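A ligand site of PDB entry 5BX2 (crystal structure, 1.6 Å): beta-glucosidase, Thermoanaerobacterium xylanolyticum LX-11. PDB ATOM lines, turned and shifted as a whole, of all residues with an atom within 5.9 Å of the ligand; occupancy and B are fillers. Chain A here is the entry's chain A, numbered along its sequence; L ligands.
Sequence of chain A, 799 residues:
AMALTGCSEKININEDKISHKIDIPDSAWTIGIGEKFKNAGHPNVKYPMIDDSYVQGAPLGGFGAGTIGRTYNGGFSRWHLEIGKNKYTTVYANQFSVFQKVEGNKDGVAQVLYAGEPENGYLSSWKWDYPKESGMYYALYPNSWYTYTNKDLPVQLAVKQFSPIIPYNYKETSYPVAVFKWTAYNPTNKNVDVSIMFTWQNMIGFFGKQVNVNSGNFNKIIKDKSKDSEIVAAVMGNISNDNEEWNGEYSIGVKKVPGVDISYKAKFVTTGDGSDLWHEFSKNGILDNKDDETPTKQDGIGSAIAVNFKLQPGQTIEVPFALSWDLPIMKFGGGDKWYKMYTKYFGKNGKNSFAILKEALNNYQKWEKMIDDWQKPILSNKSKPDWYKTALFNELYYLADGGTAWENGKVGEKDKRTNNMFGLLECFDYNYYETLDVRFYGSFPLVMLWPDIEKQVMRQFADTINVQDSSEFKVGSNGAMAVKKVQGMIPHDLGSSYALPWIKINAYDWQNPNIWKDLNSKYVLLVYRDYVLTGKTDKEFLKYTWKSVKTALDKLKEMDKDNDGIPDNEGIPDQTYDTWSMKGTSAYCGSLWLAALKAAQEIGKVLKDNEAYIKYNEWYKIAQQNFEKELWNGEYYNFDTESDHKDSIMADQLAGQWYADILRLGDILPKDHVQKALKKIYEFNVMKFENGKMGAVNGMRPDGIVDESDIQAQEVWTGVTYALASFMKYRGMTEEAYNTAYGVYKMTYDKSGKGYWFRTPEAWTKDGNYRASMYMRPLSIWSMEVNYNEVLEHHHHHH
The side-chain carboxylate of Glu 426 is covalently linked to a carbon (C1) of the ligand.
OD2 of Asp 437 sits at hydrogen-bond distance from O1 of the ligand (2.6 Å).
O of Thr 576 is in hydrogen-bond range of O2 of the ligand (2.6 Å).
OG1 of Thr 576 is in hydrogen-bond range of O2 of the ligand, 2.9 Å away.
An oxygen (O4) of the ligand is in hydrogen-bond range of the side-chain carboxylate of Glu 762, at 2.6 Å.
An oxygen (O4) of the ligand is in hydrogen-bond range of the guanidinium group (NH1) of Arg 771, 2.8 Å away.
An oxygen (O1) of the ligand is in hydrogen-bond range of a ring nitrogen (NE2) of His 492 (2.8 Å).
An oxygen (O2) of the ligand lies within hydrogen-bond range of the guanidinium group (NH2) of Arg 777, at 3.0 Å.
OE2 of Glu 426 lies within hydrogen-bond range of OH of Tyr 775, at 2.9 Å.
The backbone carbonyl oxygen (O) of Tyr 432 lies within hydrogen-bond range of the backbone NH (N) of Glu 426 (2.8 Å).
N of Glu 762 lies within hydrogen-bond range of O of Arg 771, at 3.3 Å.
OH of Tyr 775 sits at hydrogen-bond distance from OE2 of Glu 762 (3.0 Å).
NH2 of Arg 771 is in salt-bridge range of OE1 of Glu 715 (2.9 Å).
The guanidinium group (NH2) of Arg 777 sits at hydrogen-bond distance from the side-chain hydroxyl (OH) of Tyr 775.
The side-chain hydroxyl (OH) of Tyr 508 is in hydrogen-bond range of the side-chain carboxylate (OD2) of Asp 578 (2.6 Å).
OE1 of Glu 715 sits at hydrogen-bond distance from NE1 of Trp 717 (2.8 Å).
Tyr 430 touches the ligand (CD2 to O3, 3.6 Å).
Thr 435 touches the ligand (CG2 to F1, 3.7 Å).
Val 438 touches the ligand.
CD1 of Tyr 508 touches F1 of the ligand, 3.6 Å away.
Trp 516 touches the ligand.
OD1 of Asp 578 touches C6 of the ligand, 3.8 Å away.
Trp 717 touches the ligand (CH2 to C6, 3.9 Å).
OH of Tyr 775 touches C5 of the ligand (3.2 Å).
15 residues have an atom within 4 Å of the ligand: Glu 426, Tyr 430, Thr 435, Asp 437, Val 438, His 492, Tyr 508, Trp 516, Thr 576, Asp 578, Trp 717, Glu 762, Arg 771, Tyr 775 and Arg 777.
The nearest printed residue that does not touch the ligand is Gln 712 (4.1 Å).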
ATOM      1  N   GLU A 426       9.605  -6.774  -2.474  1.00  0.00           N
ATOM      2  CA  GLU A 426       9.128  -5.395  -2.543  1.00  0.00           C
ATOM      3  C   GLU A 426       8.790  -5.024  -3.984  1.00  0.00           C
ATOM      4  O   GLU A 426       7.728  -4.464  -4.260  1.00  0.00           O
ATOM      5  CB  GLU A 426      10.209  -4.462  -1.995  1.00  0.00           C
ATOM      6  CG  GLU A 426       9.806  -2.987  -1.903  1.00  0.00           C
ATOM      7  CD  GLU A 426      10.958  -2.042  -1.602  1.00  0.00           C
ATOM      8  OE1 GLU A 426      12.128  -2.459  -1.629  1.00  0.00           O
ATOM      9  OE2 GLU A 426      10.683  -0.835  -1.342  1.00  0.00           O
ATOM     10  N   TYR A 430      14.048  -2.792  -6.484  1.00  0.00           N
ATOM     11  CA  TYR A 430      14.567  -2.832  -5.130  1.00  0.00           C
ATOM     12  C   TYR A 430      14.325  -4.246  -4.619  1.00  0.00           C
ATOM     13  O   TYR A 430      13.269  -4.551  -4.075  1.00  0.00           O
ATOM     14  CB  TYR A 430      13.859  -1.805  -4.244  1.00  0.00           C
ATOM     15  CG  TYR A 430      13.517  -0.458  -4.870  1.00  0.00           C
ATOM     16  CD1 TYR A 430      14.431   0.256  -5.628  1.00  0.00           C
ATOM     17  CD2 TYR A 430      12.262   0.107  -4.666  1.00  0.00           C
ATOM     18  CE1 TYR A 430      14.115   1.495  -6.160  1.00  0.00           C
ATOM     19  CE2 TYR A 430      11.933   1.341  -5.190  1.00  0.00           C
ATOM     20  CZ  TYR A 430      12.858   2.029  -5.941  1.00  0.00           C
ATOM     21  OH  TYR A 430      12.519   3.267  -6.467  1.00  0.00           O
ATOM     22  N   TYR A 432      14.274  -6.766  -2.510  1.00  0.00           N
ATOM     23  CA  TYR A 432      14.277  -7.073  -1.073  1.00  0.00           C
ATOM     24  C   TYR A 432      13.032  -7.874  -0.725  1.00  0.00           C
ATOM     25  O   TYR A 432      11.902  -7.437  -0.992  1.00  0.00           O
ATOM     26  CB  TYR A 432      14.323  -5.770  -0.252  1.00  0.00           C
ATOM     27  CG  TYR A 432      15.516  -4.920  -0.627  1.00  0.00           C
ATOM     28  CD1 TYR A 432      16.799  -5.421  -0.519  1.00  0.00           C
ATOM     29  CD2 TYR A 432      15.354  -3.630  -1.133  1.00  0.00           C
ATOM     30  CE1 TYR A 432      17.898  -4.673  -0.882  1.00  0.00           C
ATOM     31  CE2 TYR A 432      16.456  -2.873  -1.497  1.00  0.00           C
ATOM     32  CZ  TYR A 432      17.724  -3.409  -1.375  1.00  0.00           C
ATOM     33  OH  TYR A 432      18.813  -2.638  -1.754  1.00  0.00           O
ATOM     34  N   THR A 435       9.786  -6.666   2.773  1.00  0.00           N
ATOM     35  CA  THR A 435       9.975  -5.350   3.317  1.00  0.00           C
ATOM     36  C   THR A 435       8.750  -5.073   4.190  1.00  0.00           C
ATOM     37  O   THR A 435       7.643  -4.809   3.687  1.00  0.00           O
ATOM     38  CB  THR A 435      10.130  -4.319   2.188  1.00  0.00           C
ATOM     39  OG1 THR A 435       9.073  -4.495   1.242  1.00  0.00           O
ATOM     40  CG2 THR A 435      11.418  -4.528   1.479  1.00  0.00           C
ATOM     41  N   ASP A 437       7.751  -2.754   6.222  1.00  0.00           N
ATOM     42  CA  ASP A 437       7.098  -1.455   6.178  1.00  0.00           C
ATOM     43  C   ASP A 437       6.095  -1.361   5.033  1.00  0.00           C
ATOM     44  O   ASP A 437       5.139  -0.590   5.109  1.00  0.00           O
ATOM     45  CB  ASP A 437       8.130  -0.313   6.068  1.00  0.00           C
ATOM     46  CG  ASP A 437       9.061  -0.488   4.874  1.00  0.00           C
ATOM     47  OD1 ASP A 437       9.671  -1.575   4.721  1.00  0.00           O
ATOM     48  OD2 ASP A 437       9.169   0.465   4.078  1.00  0.00           O
ATOM     49  N   VAL A 438       6.348  -2.135   3.970  1.00  0.00           N
ATOM     50  CA  VAL A 438       5.485  -2.182   2.799  1.00  0.00           C
ATOM     51  C   VAL A 438       4.424  -3.288   2.950  1.00  0.00           C
ATOM     52  O   VAL A 438       3.256  -3.110   2.534  1.00  0.00           O
ATOM     53  CB  VAL A 438       6.312  -2.435   1.508  1.00  0.00           C
ATOM     54  CG1 VAL A 438       5.422  -2.382   0.275  1.00  0.00           C
ATOM     55  CG2 VAL A 438       7.466  -1.448   1.382  1.00  0.00           C
ATOM     56  N   HIS A 492      14.073  -4.502   8.451  1.00  0.00           N
ATOM     57  CA  HIS A 492      13.383  -3.936   7.300  1.00  0.00           C
ATOM     58  C   HIS A 492      12.946  -5.009   6.316  1.00  0.00           C
ATOM     59  O   HIS A 492      11.872  -4.897   5.710  1.00  0.00           O
ATOM     60  CB  HIS A 492      14.321  -2.954   6.625  1.00  0.00           C
ATOM     61  CG  HIS A 492      13.826  -2.424   5.317  1.00  0.00           C
ATOM     62  ND1 HIS A 492      14.154  -3.016   4.113  1.00  0.00           N
ATOM     63  CD2 HIS A 492      13.077  -1.341   5.017  1.00  0.00           C
ATOM     64  CE1 HIS A 492      13.601  -2.324   3.129  1.00  0.00           C
ATOM     65  NE2 HIS A 492      12.950  -1.302   3.655  1.00  0.00           N
ATOM     66  N   TYR A 508      18.558  -4.238   2.502  1.00  0.00           N
ATOM     67  CA  TYR A 508      18.357  -2.824   2.226  1.00  0.00           C
ATOM     68  C   TYR A 508      19.351  -1.956   2.966  1.00  0.00           C
ATOM     69  O   TYR A 508      19.601  -2.145   4.167  1.00  0.00           O
ATOM     70  CB  TYR A 508      16.940  -2.467   2.633  1.00  0.00           C
ATOM     71  CG  TYR A 508      16.552  -1.006   2.637  1.00  0.00           C
ATOM     72  CD1 TYR A 508      15.988  -0.399   1.521  1.00  0.00           C
ATOM     73  CD2 TYR A 508      16.615  -0.276   3.821  1.00  0.00           C
ATOM     74  CE1 TYR A 508      15.552   0.922   1.561  1.00  0.00           C
ATOM     75  CE2 TYR A 508      16.188   1.042   3.864  1.00  0.00           C
ATOM     76  CZ  TYR A 508      15.674   1.630   2.738  1.00  0.00           C
ATOM     77  OH  TYR A 508      15.252   2.928   2.825  1.00  0.00           O
ATOM     78  N   TRP A 516      14.493   3.004  12.379  1.00  0.00           N
ATOM     79  CA  TRP A 516      13.165   3.375  11.874  1.00  0.00           C
ATOM     80  C   TRP A 516      12.132   3.398  12.984  1.00  0.00           C
ATOM     81  O   TRP A 516      12.239   2.671  13.963  1.00  0.00           O
ATOM     82  CB  TRP A 516      12.746   2.461  10.724  1.00  0.00           C
ATOM     83  CG  TRP A 516      13.384   2.860   9.428  1.00  0.00           C
ATOM     84  CD1 TRP A 516      14.540   3.585   9.263  1.00  0.00           C
ATOM     85  CD2 TRP A 516      12.909   2.564   8.116  1.00  0.00           C
ATOM     86  NE1 TRP A 516      14.801   3.758   7.933  1.00  0.00           N
ATOM     87  CE2 TRP A 516      13.815   3.125   7.197  1.00  0.00           C
ATOM     88  CE3 TRP A 516      11.792   1.865   7.616  1.00  0.00           C
ATOM     89  CZ2 TRP A 516      13.645   3.040   5.828  1.00  0.00           C
ATOM     90  CZ3 TRP A 516      11.637   1.764   6.252  1.00  0.00           C
ATOM     91  CH2 TRP A 516      12.544   2.350   5.370  1.00  0.00           C
ATOM     92  N   GLN A 575      11.524   5.918   8.190  1.00  0.00           N
ATOM     93  CA  GLN A 575      10.290   5.137   8.033  1.00  0.00           C
ATOM     94  C   GLN A 575      10.040   4.930   6.537  1.00  0.00           C
ATOM     95  O   GLN A 575      10.830   5.372   5.702  1.00  0.00           O
ATOM     96  CB  GLN A 575       9.107   5.803   8.766  1.00  0.00           C
ATOM     97  CG  GLN A 575       9.093   7.330   8.708  1.00  0.00           C
ATOM     98  CD  GLN A 575       9.041   7.884   7.305  1.00  0.00           C
ATOM     99  OE1 GLN A 575       8.237   7.410   6.491  1.00  0.00           O
ATOM    100  NE2 GLN A 575       9.861   8.896   7.007  1.00  0.00           N
ATOM    101  N   THR A 576       8.928   4.256   6.199  1.00  0.00           N
ATOM    102  CA  THR A 576       8.668   3.797   4.825  1.00  0.00           C
ATOM    103  C   THR A 576       8.797   4.862   3.727  1.00  0.00           C
ATOM    104  O   THR A 576       9.186   4.544   2.590  1.00  0.00           O
ATOM    105  CB  THR A 576       7.280   3.114   4.740  1.00  0.00           C
ATOM    106  OG1 THR A 576       7.219   2.237   3.601  1.00  0.00           O
ATOM    107  CG2 THR A 576       6.142   4.126   4.705  1.00  0.00           C
ATOM    108  N   TYR A 577       8.484   6.121   4.043  1.00  0.00           N
ATOM    109  CA  TYR A 577       8.691   7.205   3.109  1.00  0.00           C
ATOM    110  C   TYR A 577      10.163   7.569   3.229  1.00  0.00           C
ATOM    111  O   TYR A 577      10.529   8.551   3.898  1.00  0.00           O
ATOM    112  CB  TYR A 577       7.759   8.387   3.398  1.00  0.00           C
ATOM    113  CG  TYR A 577       6.276   8.040   3.304  1.00  0.00           C
ATOM    114  CD1 TYR A 577       5.579   7.536   4.402  1.00  0.00           C
ATOM    115  CD2 TYR A 577       5.581   8.194   2.097  1.00  0.00           C
ATOM    116  CE1 TYR A 577       4.230   7.204   4.317  1.00  0.00           C
ATOM    117  CE2 TYR A 577       4.229   7.884   2.008  1.00  0.00           C
ATOM    118  CZ  TYR A 577       3.554   7.383   3.109  1.00  0.00           C
ATOM    119  OH  TYR A 577       2.215   7.099   3.007  1.00  0.00           O
ATOM    120  N   ASP A 578      10.996   6.746   2.598  1.00  0.00           N
ATOM    121  CA  ASP A 578      12.424   6.685   2.914  1.00  0.00           C
ATOM    122  C   ASP A 578      13.287   7.759   2.233  1.00  0.00           C
ATOM    123  O   ASP A 578      14.512   7.681   2.262  1.00  0.00           O
ATOM    124  CB  ASP A 578      12.983   5.266   2.695  1.00  0.00           C
ATOM    125  CG  ASP A 578      13.036   4.859   1.220  1.00  0.00           C
ATOM    126  OD1 ASP A 578      12.470   5.558   0.356  1.00  0.00           O
ATOM    127  OD2 ASP A 578      13.655   3.797   0.921  1.00  0.00           O
ATOM    128  N   GLN A 712       8.782  12.164  -2.792  1.00  0.00           N
ATOM    129  CA  GLN A 712       7.715  11.289  -2.290  1.00  0.00           C
ATOM    130  C   GLN A 712       6.466  12.055  -1.882  1.00  0.00           C
ATOM    131  O   GLN A 712       5.359  11.530  -1.998  1.00  0.00           O
ATOM    132  CB  GLN A 712       8.215  10.397  -1.148  1.00  0.00           C
ATOM    133  CG  GLN A 712       9.209   9.355  -1.635  1.00  0.00           C
ATOM    134  CD  GLN A 712       9.835   8.563  -0.509  1.00  0.00           C
ATOM    135  OE1 GLN A 712       9.784   8.938   0.663  1.00  0.00           O
ATOM    136  NE2 GLN A 712      10.427   7.418  -0.871  1.00  0.00           N
ATOM    137  N   GLU A 715       4.305  12.361  -4.987  1.00  0.00           N
ATOM    138  CA  GLU A 715       3.888  11.105  -5.578  1.00  0.00           C
ATOM    139  C   GLU A 715       2.549  10.664  -5.007  1.00  0.00           C
ATOM    140  O   GLU A 715       2.244  10.879  -3.830  1.00  0.00           O
ATOM    141  CB  GLU A 715       4.921  10.007  -5.310  1.00  0.00           C
ATOM    142  CG  GLU A 715       6.223  10.138  -6.114  1.00  0.00           C
ATOM    143  CD  GLU A 715       7.246   9.049  -5.788  1.00  0.00           C
ATOM    144  OE1 GLU A 715       7.288   8.547  -4.641  1.00  0.00           O
ATOM    145  OE2 GLU A 715       8.025   8.692  -6.689  1.00  0.00           O
ATOM    146  N   TRP A 717       1.050   7.197  -4.017  1.00  0.00           N
ATOM    147  CA  TRP A 717       1.454   5.821  -3.766  1.00  0.00           C
ATOM    148  C   TRP A 717       0.189   4.969  -3.895  1.00  0.00           C
ATOM    149  O   TRP A 717      -0.764   5.140  -3.146  1.00  0.00           O
ATOM    150  CB  TRP A 717       2.123   5.661  -2.398  1.00  0.00           C
ATOM    151  CG  TRP A 717       3.561   6.135  -2.383  1.00  0.00           C
ATOM    152  CD1 TRP A 717       4.165   6.952  -3.290  1.00  0.00           C
ATOM    153  CD2 TRP A 717       4.554   5.823  -1.399  1.00  0.00           C
ATOM    154  NE1 TRP A 717       5.467   7.168  -2.938  1.00  0.00           N
ATOM    155  CE2 TRP A 717       5.735   6.484  -1.785  1.00  0.00           C
ATOM    156  CE3 TRP A 717       4.572   5.064  -0.224  1.00  0.00           C
ATOM    157  CZ2 TRP A 717       6.921   6.407  -1.044  1.00  0.00           C
ATOM    158  CZ3 TRP A 717       5.754   4.966   0.500  1.00  0.00           C
ATOM    159  CH2 TRP A 717       6.904   5.647   0.094  1.00  0.00           C
ATOM    160  N   GLU A 762       4.764   1.350  -7.498  1.00  0.00           N
ATOM    161  CA  GLU A 762       4.663   2.045  -6.222  1.00  0.00           C
ATOM    162  C   GLU A 762       3.948   3.386  -6.406  1.00  0.00           C
ATOM    163  O   GLU A 762       3.008   3.688  -5.696  1.00  0.00           O
ATOM    164  CB  GLU A 762       6.053   2.316  -5.638  1.00  0.00           C
ATOM    165  CG  GLU A 762       6.091   3.301  -4.469  1.00  0.00           C
ATOM    166  CD  GLU A 762       5.825   2.681  -3.107  1.00  0.00           C
ATOM    167  OE1 GLU A 762       4.656   2.330  -2.811  1.00  0.00           O
ATOM    168  OE2 GLU A 762       6.779   2.602  -2.301  1.00  0.00           O
ATOM    169  N   ARG A 771       7.374   5.323 -10.658  1.00  0.00           N
ATOM    170  CA  ARG A 771       8.539   4.741 -10.001  1.00  0.00           C
ATOM    171  C   ARG A 771       8.188   3.344  -9.511  1.00  0.00           C
ATOM    172  O   ARG A 771       7.193   3.161  -8.803  1.00  0.00           O
ATOM    173  CB  ARG A 771       8.987   5.623  -8.840  1.00  0.00           C
ATOM    174  CG  ARG A 771      10.226   5.117  -8.102  1.00  0.00           C
ATOM    175  CD  ARG A 771      10.765   6.179  -7.151  1.00  0.00           C
ATOM    176  NE  ARG A 771       9.837   6.503  -6.073  1.00  0.00           N
ATOM    177  CZ  ARG A 771       9.653   5.759  -4.986  1.00  0.00           C
ATOM    178  NH1 ARG A 771      10.324   4.616  -4.821  1.00  0.00           N
ATOM    179  NH2 ARG A 771       8.779   6.132  -4.071  1.00  0.00           N
ATOM    180  N   TYR A 775       4.999  -3.831  -8.087  1.00  0.00           N
ATOM    181  CA  TYR A 775       5.230  -3.393  -6.715  1.00  0.00           C
ATOM    182  C   TYR A 775       4.272  -4.043  -5.708  1.00  0.00           C
ATOM    183  O   TYR A 775       3.125  -4.281  -6.011  1.00  0.00           O
ATOM    184  CB  TYR A 775       5.144  -1.858  -6.632  1.00  0.00           C
ATOM    185  CG  TYR A 775       5.883  -1.352  -5.433  1.00  0.00           C
ATOM    186  CD1 TYR A 775       7.269  -1.280  -5.444  1.00  0.00           C
ATOM    187  CD2 TYR A 775       5.222  -0.993  -4.277  1.00  0.00           C
ATOM    188  CE1 TYR A 775       7.970  -0.876  -4.337  1.00  0.00           C
ATOM    189  CE2 TYR A 775       5.926  -0.599  -3.148  1.00  0.00           C
ATOM    190  CZ  TYR A 775       7.300  -0.547  -3.187  1.00  0.00           C
ATOM    191  OH  TYR A 775       7.990  -0.157  -2.050  1.00  0.00           O
ATOM    192  N   ARG A 777       3.027  -2.991  -2.667  1.00  0.00           N
ATOM    193  CA  ARG A 777       2.085  -2.225  -1.838  1.00  0.00           C
ATOM    194  C   ARG A 777       0.614  -2.206  -2.319  1.00  0.00           C
ATOM    195  O   ARG A 777      -0.272  -2.277  -1.478  1.00  0.00           O
ATOM    196  CB  ARG A 777       2.578  -0.797  -1.602  1.00  0.00           C
ATOM    197  CG  ARG A 777       2.238  -0.227  -0.232  1.00  0.00           C
ATOM    198  CD  ARG A 777       2.700   1.227  -0.056  1.00  0.00           C
ATOM    199  NE  ARG A 777       4.143   1.416  -0.281  1.00  0.00           N
ATOM    200  CZ  ARG A 777       5.088   1.496   0.672  1.00  0.00           C
ATOM    201  NH1 ARG A 777       4.779   1.379   1.965  1.00  0.00           N
ATOM    202  NH2 ARG A 777       6.356   1.709   0.343  1.00  0.00           N
HETATM  203  C1  LIG L   1      11.606   0.126  -1.112  1.00  0.00           C
HETATM  204  C2  LIG L   1      12.044   0.160   0.340  1.00  0.00           C
HETATM  205  C3  LIG L   1      10.858   0.552   1.221  1.00  0.00           C
HETATM  206  C4  LIG L   1      10.329   1.913   0.777  1.00  0.00           C
HETATM  207  C5  LIG L   1      10.066   1.968  -0.733  1.00  0.00           C
HETATM  208  C6  LIG L   1       9.806   3.409  -1.187  1.00  0.00           C
HETATM  209  O1  LIG L   1      11.255   0.636   2.596  1.00  0.00           O
HETATM  210  O2  LIG L   1       9.106   2.190   1.444  1.00  0.00           O
HETATM  211  O3  LIG L   1      11.140   1.413  -1.523  1.00  0.00           O
HETATM  212  O4  LIG L   1       9.274   3.455  -2.524  1.00  0.00           O
HETATM  213  F1  LIG L   1      12.540  -1.054   0.734  1.00  0.00           F
